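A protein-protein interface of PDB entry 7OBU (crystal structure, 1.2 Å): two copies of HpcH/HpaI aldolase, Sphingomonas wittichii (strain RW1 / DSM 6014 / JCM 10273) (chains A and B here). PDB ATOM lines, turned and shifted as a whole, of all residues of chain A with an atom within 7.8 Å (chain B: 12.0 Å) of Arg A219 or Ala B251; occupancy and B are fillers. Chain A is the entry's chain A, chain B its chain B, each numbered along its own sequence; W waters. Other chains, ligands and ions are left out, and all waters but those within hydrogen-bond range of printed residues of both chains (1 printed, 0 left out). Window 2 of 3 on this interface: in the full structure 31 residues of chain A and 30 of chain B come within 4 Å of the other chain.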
ATOM      1  N   LEU A  16      -0.932 -30.375  -6.073  1.00  0.00           N
ATOM      2  CA  LEU A  16      -1.162 -30.613  -4.656  1.00  0.00           C
ATOM      3  C   LEU A  16      -2.639 -30.912  -4.468  1.00  0.00           C
ATOM      4  O   LEU A  16      -3.496 -30.182  -4.985  1.00  0.00           O
ATOM      5  CB  LEU A  16      -0.791 -29.388  -3.814  1.00  0.00           C
ATOM      6  CG  LEU A  16      -0.980 -29.557  -2.300  1.00  0.00           C
ATOM      7  CD1 LEU A  16       0.056 -30.510  -1.713  1.00  0.00           C
ATOM      8  CD2 LEU A  16      -0.882 -28.222  -1.574  1.00  0.00           C
ATOM      9  N   CYS A 212       0.826 -37.967   1.703  1.00  0.00           N
ATOM     10  CA  CYS A 212       1.476 -37.332   2.839  1.00  0.00           C
ATOM     11  C   CYS A 212       0.495 -37.064   3.969  1.00  0.00           C
ATOM     12  O   CYS A 212      -0.694 -36.819   3.747  1.00  0.00           O
ATOM     13  CB  CYS A 212       2.159 -36.012   2.467  1.00  0.00           C
ATOM     14  SG  CYS A 212       3.269 -36.141   1.063  1.00  0.00           S
ATOM     15  N   SER A 214       1.161 -34.636   6.344  1.00  0.00           N
ATOM     16  CA  SER A 214       1.480 -33.345   6.918  1.00  0.00           C
ATOM     17  C   SER A 214       1.924 -32.417   5.807  1.00  0.00           C
ATOM     18  O   SER A 214       2.436 -32.855   4.773  1.00  0.00           O
ATOM     19  CB  SER A 214       2.614 -33.464   7.935  1.00  0.00           C
ATOM     20  OG  SER A 214       3.778 -33.991   7.322  1.00  0.00           O
ATOM     21  N   GLY A 215       1.788 -31.122   6.069  1.00  0.00           N
ATOM     22  CA  GLY A 215       2.284 -30.137   5.130  1.00  0.00           C
ATOM     23  C   GLY A 215       3.792 -30.154   5.013  1.00  0.00           C
ATOM     24  O   GLY A 215       4.336 -29.953   3.926  1.00  0.00           O
ATOM     25  N   GLY A 216       4.488 -30.401   6.122  1.00  0.00           N
ATOM     26  CA  GLY A 216       5.936 -30.414   6.071  1.00  0.00           C
ATOM     27  C   GLY A 216       6.480 -31.546   5.228  1.00  0.00           C
ATOM     28  O   GLY A 216       7.448 -31.367   4.490  1.00  0.00           O
ATOM     29  N   PHE A 217       5.897 -32.738   5.353  1.00  0.00           N
ATOM     30  CA  PHE A 217       6.376 -33.856   4.550  1.00  0.00           C
ATOM     31  C   PHE A 217       6.051 -33.604   3.079  1.00  0.00           C
ATOM     32  O   PHE A 217       6.894 -33.856   2.200  1.00  0.00           O
ATOM     33  CB  PHE A 217       5.783 -35.169   5.081  1.00  0.00           C
ATOM     34  CG  PHE A 217       6.388 -36.422   4.469  1.00  0.00           C
ATOM     35  CD1 PHE A 217       7.530 -36.980   4.998  1.00  0.00           C
ATOM     36  CD2 PHE A 217       5.770 -37.070   3.414  1.00  0.00           C
ATOM     37  CE1 PHE A 217       8.083 -38.141   4.446  1.00  0.00           C
ATOM     38  CE2 PHE A 217       6.305 -38.216   2.880  1.00  0.00           C
ATOM     39  CZ  PHE A 217       7.461 -38.750   3.401  1.00  0.00           C
ATOM     40  N   ALA A 218       4.854 -33.059   2.796  1.00  0.00           N
ATOM     41  CA  ALA A 218       4.482 -32.710   1.427  1.00  0.00           C
ATOM     42  C   ALA A 218       5.458 -31.709   0.824  1.00  0.00           C
ATOM     43  O   ALA A 218       5.835 -31.827  -0.351  1.00  0.00           O
ATOM     44  CB  ALA A 218       3.071 -32.132   1.415  1.00  0.00           C
ATOM     45  N   ARG A 219       5.900 -30.722   1.613  1.00  0.00           N
ATOM     46  CA  ARG A 219       6.866 -29.754   1.112  1.00  0.00           C
ATOM     47  C   ARG A 219       8.139 -30.445   0.656  1.00  0.00           C
ATOM     48  O   ARG A 219       8.681 -30.116  -0.405  1.00  0.00           O
ATOM     49  CB  ARG A 219       7.162 -28.739   2.204  1.00  0.00           C
ATOM     50  CG  ARG A 219       8.123 -27.630   1.819  1.00  0.00           C
ATOM     51  CD  ARG A 219       8.436 -26.776   3.048  1.00  0.00           C
ATOM     52  NE  ARG A 219       9.273 -25.621   2.733  1.00  0.00           N
ATOM     53  CZ  ARG A 219       9.085 -24.396   3.213  1.00  0.00           C
ATOM     54  NH1 ARG A 219       8.099 -24.121   4.055  1.00  0.00           N
ATOM     55  NH2 ARG A 219       9.916 -23.423   2.848  1.00  0.00           N
ATOM     56  N   VAL A 220       8.632 -31.398   1.440  1.00  0.00           N
ATOM     57  CA  VAL A 220       9.844 -32.112   1.053  1.00  0.00           C
ATOM     58  C   VAL A 220       9.603 -32.911  -0.216  1.00  0.00           C
ATOM     59  O   VAL A 220      10.438 -32.943  -1.116  1.00  0.00           O
ATOM     60  CB  VAL A 220      10.346 -32.997   2.206  1.00  0.00           C
ATOM     61  CG1 VAL A 220      11.558 -33.803   1.753  1.00  0.00           C
ATOM     62  CG2 VAL A 220      10.657 -32.139   3.412  1.00  0.00           C
ATOM     63  N   LYS A 221       8.471 -33.617  -0.285  1.00  0.00           N
ATOM     64  CA  LYS A 221       8.182 -34.427  -1.480  1.00  0.00           C
ATOM     65  C   LYS A 221       8.091 -33.558  -2.738  1.00  0.00           C
ATOM     66  O   LYS A 221       8.610 -33.926  -3.799  1.00  0.00           O
ATOM     67  CB  LYS A 221       6.912 -35.254  -1.294  1.00  0.00           C
ATOM     68  CG  LYS A 221       6.952 -36.246  -0.137  1.00  0.00           C
ATOM     69  CD  LYS A 221       8.137 -37.163  -0.107  1.00  0.00           C
ATOM     70  CE  LYS A 221       9.152 -36.694   0.925  1.00  0.00           C
ATOM     71  NZ  LYS A 221      10.272 -37.652   0.952  1.00  0.00           N
ATOM     72  N   LEU A 222       7.451 -32.397  -2.642  1.00  0.00           N
ATOM     73  CA  LEU A 222       7.462 -31.476  -3.772  1.00  0.00           C
ATOM     74  C   LEU A 222       8.891 -31.090  -4.141  1.00  0.00           C
ATOM     75  O   LEU A 222       9.245 -31.089  -5.319  1.00  0.00           O
ATOM     76  CB  LEU A 222       6.594 -30.269  -3.448  1.00  0.00           C
ATOM     77  CG  LEU A 222       5.100 -30.590  -3.360  1.00  0.00           C
ATOM     78  CD1 LEU A 222       4.376 -29.492  -2.607  1.00  0.00           C
ATOM     79  CD2 LEU A 222       4.502 -30.778  -4.745  1.00  0.00           C
ATOM     80  N   ALA A 223       9.742 -30.802  -3.141  1.00  0.00           N
ATOM     81  CA  ALA A 223      11.145 -30.433  -3.421  1.00  0.00           C
ATOM     82  C   ALA A 223      11.932 -31.575  -4.066  1.00  0.00           C
ATOM     83  O   ALA A 223      12.897 -31.325  -4.802  1.00  0.00           O
ATOM     84  CB  ALA A 223      11.840 -29.983  -2.132  1.00  0.00           C
ATOM     85  N   GLU A 224      11.565 -32.831  -3.756  1.00  0.00           N
ATOM     86  CA  GLU A 224      12.203 -34.012  -4.325  1.00  0.00           C
ATOM     87  C   GLU A 224      11.716 -34.303  -5.740  1.00  0.00           C
ATOM     88  O   GLU A 224      12.240 -35.219  -6.384  1.00  0.00           O
ATOM     89  CB  GLU A 224      11.943 -35.217  -3.411  1.00  0.00           C
ATOM     90  CG  GLU A 224      12.753 -35.152  -2.126  1.00  0.00           C
ATOM     91  CD  GLU A 224      12.608 -36.349  -1.231  1.00  0.00           C
ATOM     92  OE1 GLU A 224      11.613 -37.094  -1.382  1.00  0.00           O
ATOM     93  OE2 GLU A 224      13.521 -36.557  -0.398  1.00  0.00           O
ATOM     94  N   GLY A 225      10.772 -33.522  -6.259  1.00  0.00           N
ATOM     95  CA  GLY A 225      10.339 -33.661  -7.629  1.00  0.00           C
ATOM     96  C   GLY A 225       9.102 -34.503  -7.855  1.00  0.00           C
ATOM     97  O   GLY A 225       8.803 -34.833  -9.003  1.00  0.00           O
ATOM     98  N   VAL A 229       1.097 -34.693  -5.037  1.00  0.00           N
ATOM     99  CA  VAL A 229       1.369 -34.833  -3.610  1.00  0.00           C
ATOM    100  C   VAL A 229       0.065 -34.548  -2.903  1.00  0.00           C
ATOM    101  O   VAL A 229      -0.582 -33.544  -3.203  1.00  0.00           O
ATOM    102  CB  VAL A 229       2.482 -33.849  -3.178  1.00  0.00           C
ATOM    103  CG1 VAL A 229       2.700 -33.865  -1.701  1.00  0.00           C
ATOM    104  CG2 VAL A 229       3.768 -34.200  -3.903  1.00  0.00           C
ATOM    105  N   ALA A 231      -1.953 -33.961   0.771  1.00  0.00           N
ATOM    106  CA  ALA A 231      -1.773 -33.630   2.178  1.00  0.00           C
ATOM    107  C   ALA A 231      -2.946 -32.785   2.650  1.00  0.00           C
ATOM    108  O   ALA A 231      -3.347 -31.865   1.936  1.00  0.00           O
ATOM    109  CB  ALA A 231      -0.493 -32.815   2.369  1.00  0.00           C
ATOM    110  N   ALA B 242      -6.533 -27.118   6.883  1.00  0.00           N
ATOM    111  CA  ALA B 242      -6.170 -27.347   5.491  1.00  0.00           C
ATOM    112  C   ALA B 242      -5.409 -26.159   4.909  1.00  0.00           C
ATOM    113  O   ALA B 242      -4.439 -26.347   4.170  1.00  0.00           O
ATOM    114  CB  ALA B 242      -7.419 -27.683   4.681  1.00  0.00           C
ATOM    115  N   ARG B 243      -5.857 -24.934   5.196  1.00  0.00           N
ATOM    116  CA  ARG B 243      -5.148 -23.767   4.681  1.00  0.00           C
ATOM    117  C   ARG B 243      -3.703 -23.763   5.152  1.00  0.00           C
ATOM    118  O   ARG B 243      -2.792 -23.403   4.385  1.00  0.00           O
ATOM    119  CB  ARG B 243      -5.857 -22.486   5.121  1.00  0.00           C
ATOM    120  CG  ARG B 243      -7.125 -22.210   4.346  1.00  0.00           C
ATOM    121  CD  ARG B 243      -7.711 -20.817   4.601  1.00  0.00           C
ATOM    122  NE  ARG B 243      -8.030 -20.568   6.003  1.00  0.00           N
ATOM    123  CZ  ARG B 243      -9.190 -20.870   6.578  1.00  0.00           C
ATOM    124  NH1 ARG B 243     -10.155 -21.469   5.911  1.00  0.00           N
ATOM    125  NH2 ARG B 243      -9.377 -20.581   7.862  1.00  0.00           N
ATOM    126  N   GLN B 244      -3.480 -24.152   6.408  1.00  0.00           N
ATOM    127  CA  GLN B 244      -2.124 -24.173   6.953  1.00  0.00           C
ATOM    128  C   GLN B 244      -1.292 -25.276   6.305  1.00  0.00           C
ATOM    129  O   GLN B 244      -0.109 -25.065   6.006  1.00  0.00           O
ATOM    130  CB  GLN B 244      -2.147 -24.335   8.478  1.00  0.00           C
ATOM    131  CG  GLN B 244      -0.761 -24.232   9.121  1.00  0.00           C
ATOM    132  CD  GLN B 244      -0.142 -22.866   8.907  1.00  0.00           C
ATOM    133  OE1 GLN B 244      -0.697 -21.858   9.351  1.00  0.00           O
ATOM    134  NE2 GLN B 244       1.009 -22.819   8.216  1.00  0.00           N
ATOM    135  N   VAL B 245      -1.884 -26.459   6.088  1.00  0.00           N
ATOM    136  CA  VAL B 245      -1.157 -27.532   5.412  1.00  0.00           C
ATOM    137  C   VAL B 245      -0.738 -27.090   4.019  1.00  0.00           C
ATOM    138  O   VAL B 245       0.384 -27.355   3.583  1.00  0.00           O
ATOM    139  CB  VAL B 245      -2.019 -28.808   5.374  1.00  0.00           C
ATOM    140  CG1 VAL B 245      -1.503 -29.790   4.334  1.00  0.00           C
ATOM    141  CG2 VAL B 245      -2.056 -29.442   6.732  1.00  0.00           C
ATOM    142  N   ILE B 246      -1.641 -26.440   3.289  1.00  0.00           N
ATOM    143  CA  ILE B 246      -1.341 -25.982   1.938  1.00  0.00           C
ATOM    144  C   ILE B 246      -0.226 -24.951   1.960  1.00  0.00           C
ATOM    145  O   ILE B 246       0.697 -25.006   1.146  1.00  0.00           O
ATOM    146  CB  ILE B 246      -2.613 -25.434   1.273  1.00  0.00           C
ATOM    147  CG1 ILE B 246      -3.585 -26.568   0.976  1.00  0.00           C
ATOM    148  CG2 ILE B 246      -2.262 -24.695   0.023  1.00  0.00           C
ATOM    149  CD1 ILE B 246      -4.987 -26.100   0.665  1.00  0.00           C
ATOM    150  N   ALA B 247      -0.308 -23.983   2.876  1.00  0.00           N
ATOM    151  CA  ALA B 247       0.748 -22.981   2.973  1.00  0.00           C
ATOM    152  C   ALA B 247       2.088 -23.632   3.280  1.00  0.00           C
ATOM    153  O   ALA B 247       3.121 -23.226   2.721  1.00  0.00           O
ATOM    154  CB  ALA B 247       0.379 -21.953   4.044  1.00  0.00           C
ATOM    155  N   ASP B 248       2.101 -24.604   4.190  1.00  0.00           N
ATOM    156  CA  ASP B 248       3.347 -25.290   4.515  1.00  0.00           C
ATOM    157  C   ASP B 248       3.875 -26.044   3.293  1.00  0.00           C
ATOM    158  O   ASP B 248       5.059 -25.981   2.957  1.00  0.00           O
ATOM    159  CB  ASP B 248       3.180 -26.238   5.719  1.00  0.00           C
ATOM    160  CG  ASP B 248       2.809 -25.525   7.020  1.00  0.00           C
ATOM    161  OD1 ASP B 248       2.944 -24.295   7.088  1.00  0.00           O
ATOM    162  OD2 ASP B 248       2.456 -26.225   8.001  1.00  0.00           O
ATOM    163  N   ALA B 249       3.003 -26.766   2.600  1.00  0.00           N
ATOM    164  CA  ALA B 249       3.451 -27.581   1.477  1.00  0.00           C
ATOM    165  C   ALA B 249       4.004 -26.727   0.358  1.00  0.00           C
ATOM    166  O   ALA B 249       4.987 -27.093  -0.296  1.00  0.00           O
ATOM    167  CB  ALA B 249       2.264 -28.370   0.938  1.00  0.00           C
ATOM    168  N   ARG B 250       3.332 -25.629   0.067  1.00  0.00           N
ATOM    169  CA  ARG B 250       3.664 -24.764  -1.049  1.00  0.00           C
ATOM    170  C   ARG B 250       4.758 -23.772  -0.686  1.00  0.00           C
ATOM    171  O   ARG B 250       5.178 -23.005  -1.552  1.00  0.00           O
ATOM    172  CB  ARG B 250       2.400 -24.044  -1.524  1.00  0.00           C
ATOM    173  CG  ARG B 250       1.342 -24.986  -2.163  1.00  0.00           C
ATOM    174  CD  ARG B 250       0.405 -24.208  -3.038  1.00  0.00           C
ATOM    175  NE  ARG B 250      -0.685 -24.980  -3.615  1.00  0.00           N
ATOM    176  CZ  ARG B 250      -0.597 -25.646  -4.761  1.00  0.00           C
ATOM    177  NH1 ARG B 250       0.550 -25.767  -5.405  1.00  0.00           N
ATOM    178  NH2 ARG B 250      -1.691 -26.170  -5.296  1.00  0.00           N
ATOM    179  N   ALA B 251       5.220 -23.791   0.568  1.00  0.00           N
ATOM    180  CA  ALA B 251       6.297 -22.920   1.049  1.00  0.00           C
ATOM    181  C   ALA B 251       5.876 -21.459   0.987  1.00  0.00           C
ATOM    182  O   ALA B 251       6.595 -20.590   0.484  1.00  0.00           O
ATOM    183  CB  ALA B 251       7.602 -23.181   0.304  1.00  0.00           C
ATOM    184  N   LEU B 252       4.698 -21.194   1.536  1.00  0.00           N
ATOM    185  CA  LEU B 252       4.116 -19.861   1.517  1.00  0.00           C
ATOM    186  C   LEU B 252       3.928 -19.341   2.932  1.00  0.00           C
ATOM    187  O   LEU B 252       4.173 -20.060   3.906  1.00  0.00           O
ATOM    188  CB  LEU B 252       2.787 -19.924   0.765  1.00  0.00           C
ATOM    189  CG  LEU B 252       2.936 -20.109  -0.751  1.00  0.00           C
ATOM    190  CD1 LEU B 252       1.579 -20.084  -1.439  1.00  0.00           C
ATOM    191  CD2 LEU B 252       3.865 -19.044  -1.361  1.00  0.00           C
ATOM    192  OXT LEU B 252       3.549 -18.185   3.131  1.00  0.00           O
HETATM  193  O   HOH W   1       6.341 -21.714   4.503  1.00  0.00           O
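The side-chain amide nitrogen (NE2) of Gln B244 is in hydrogen-bond range of the side-chain carboxylate (OD1) of Asp B248 (2.7 Å).
Arg B250 touches Leu A16.
Val B245 touches Gly A215.
O of Gly A215 touches C of Asp B248, 3.99 Å away.
Gly A215 touches Ala B249.
CB of Ala A218 touches CB of Ala B249, at 3.9 Å.
Asp B248 touches Arg A219.
CA of Arg A219 touches O of Ala B249, at 3.5 Å.
Ala B251 touches Arg A219 (CB to NH2, 3.4 Å).
Leu A222 touches Ala B249.
O of Ala A231 touches CG1 of Val B245, at 3.7 Å.
Printed residues of chain B within 4 Å of Leu A16: Arg B250 (3.7 Å).
Ser A214 touches none of the printed residues of chain B.
Printed residues of chain B within 4 Å of Gly A215: Val B245, Asp B248 and Ala B249.
Of chain B, only Ala B249 comes within 4 Å of Ala A218.
Of chain B, only Asp B248 (3.5 Å), Ala B249 (3.5 Å) and Ala B251 (3.4 Å) come within 4 Å of Arg A219.
No residue of chain B comes within 4 Å of Val A220.
No residue of chain B comes within 4 Å of Ala A223.
Glu A224 touches none of the printed residues of chain B.
Printed residues of chain B within 4 Å of Ala A231: Val B245.
Of the printed residues of chain A, Ala B249 touches Gly A215 (3.5 Å), Ala A218 (3.9 Å), Arg A219 (3.5 Å) and Leu A222 (3.4 Å).
Printed residues of chain A within 4 Å of Arg B250: Leu A16 (3.7 Å).
Ala B251 touches just one residue of chain A: Arg A219 (3.4 Å).
Leu B252 touches none of the printed residues of chain A.
The nearest residue of chain A that does not touch Ala B251 is Leu A222 (6.6 Å).
Of the 16 printed residues of chain A, 6 touch a printed residue of chain B.
Hydrophobic or aromatic side chains of chain A that line the printed part of chain B: Leu A16, Ala A218, Leu A222 and Ala A231.
Hydrophobic or aromatic side chains of chain B that line the printed part of chain A: Val B245, Ala B249 and Ala B251.
Among the printed residues, 10 pairs touch across the chains.
No position is printed for both chains.
Water W1 lies within hydrogen-bond range of the chain-end carboxylate of Leu B252 (2.8 Å) and the guanidinium group of Arg A219 (3.0 Å).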
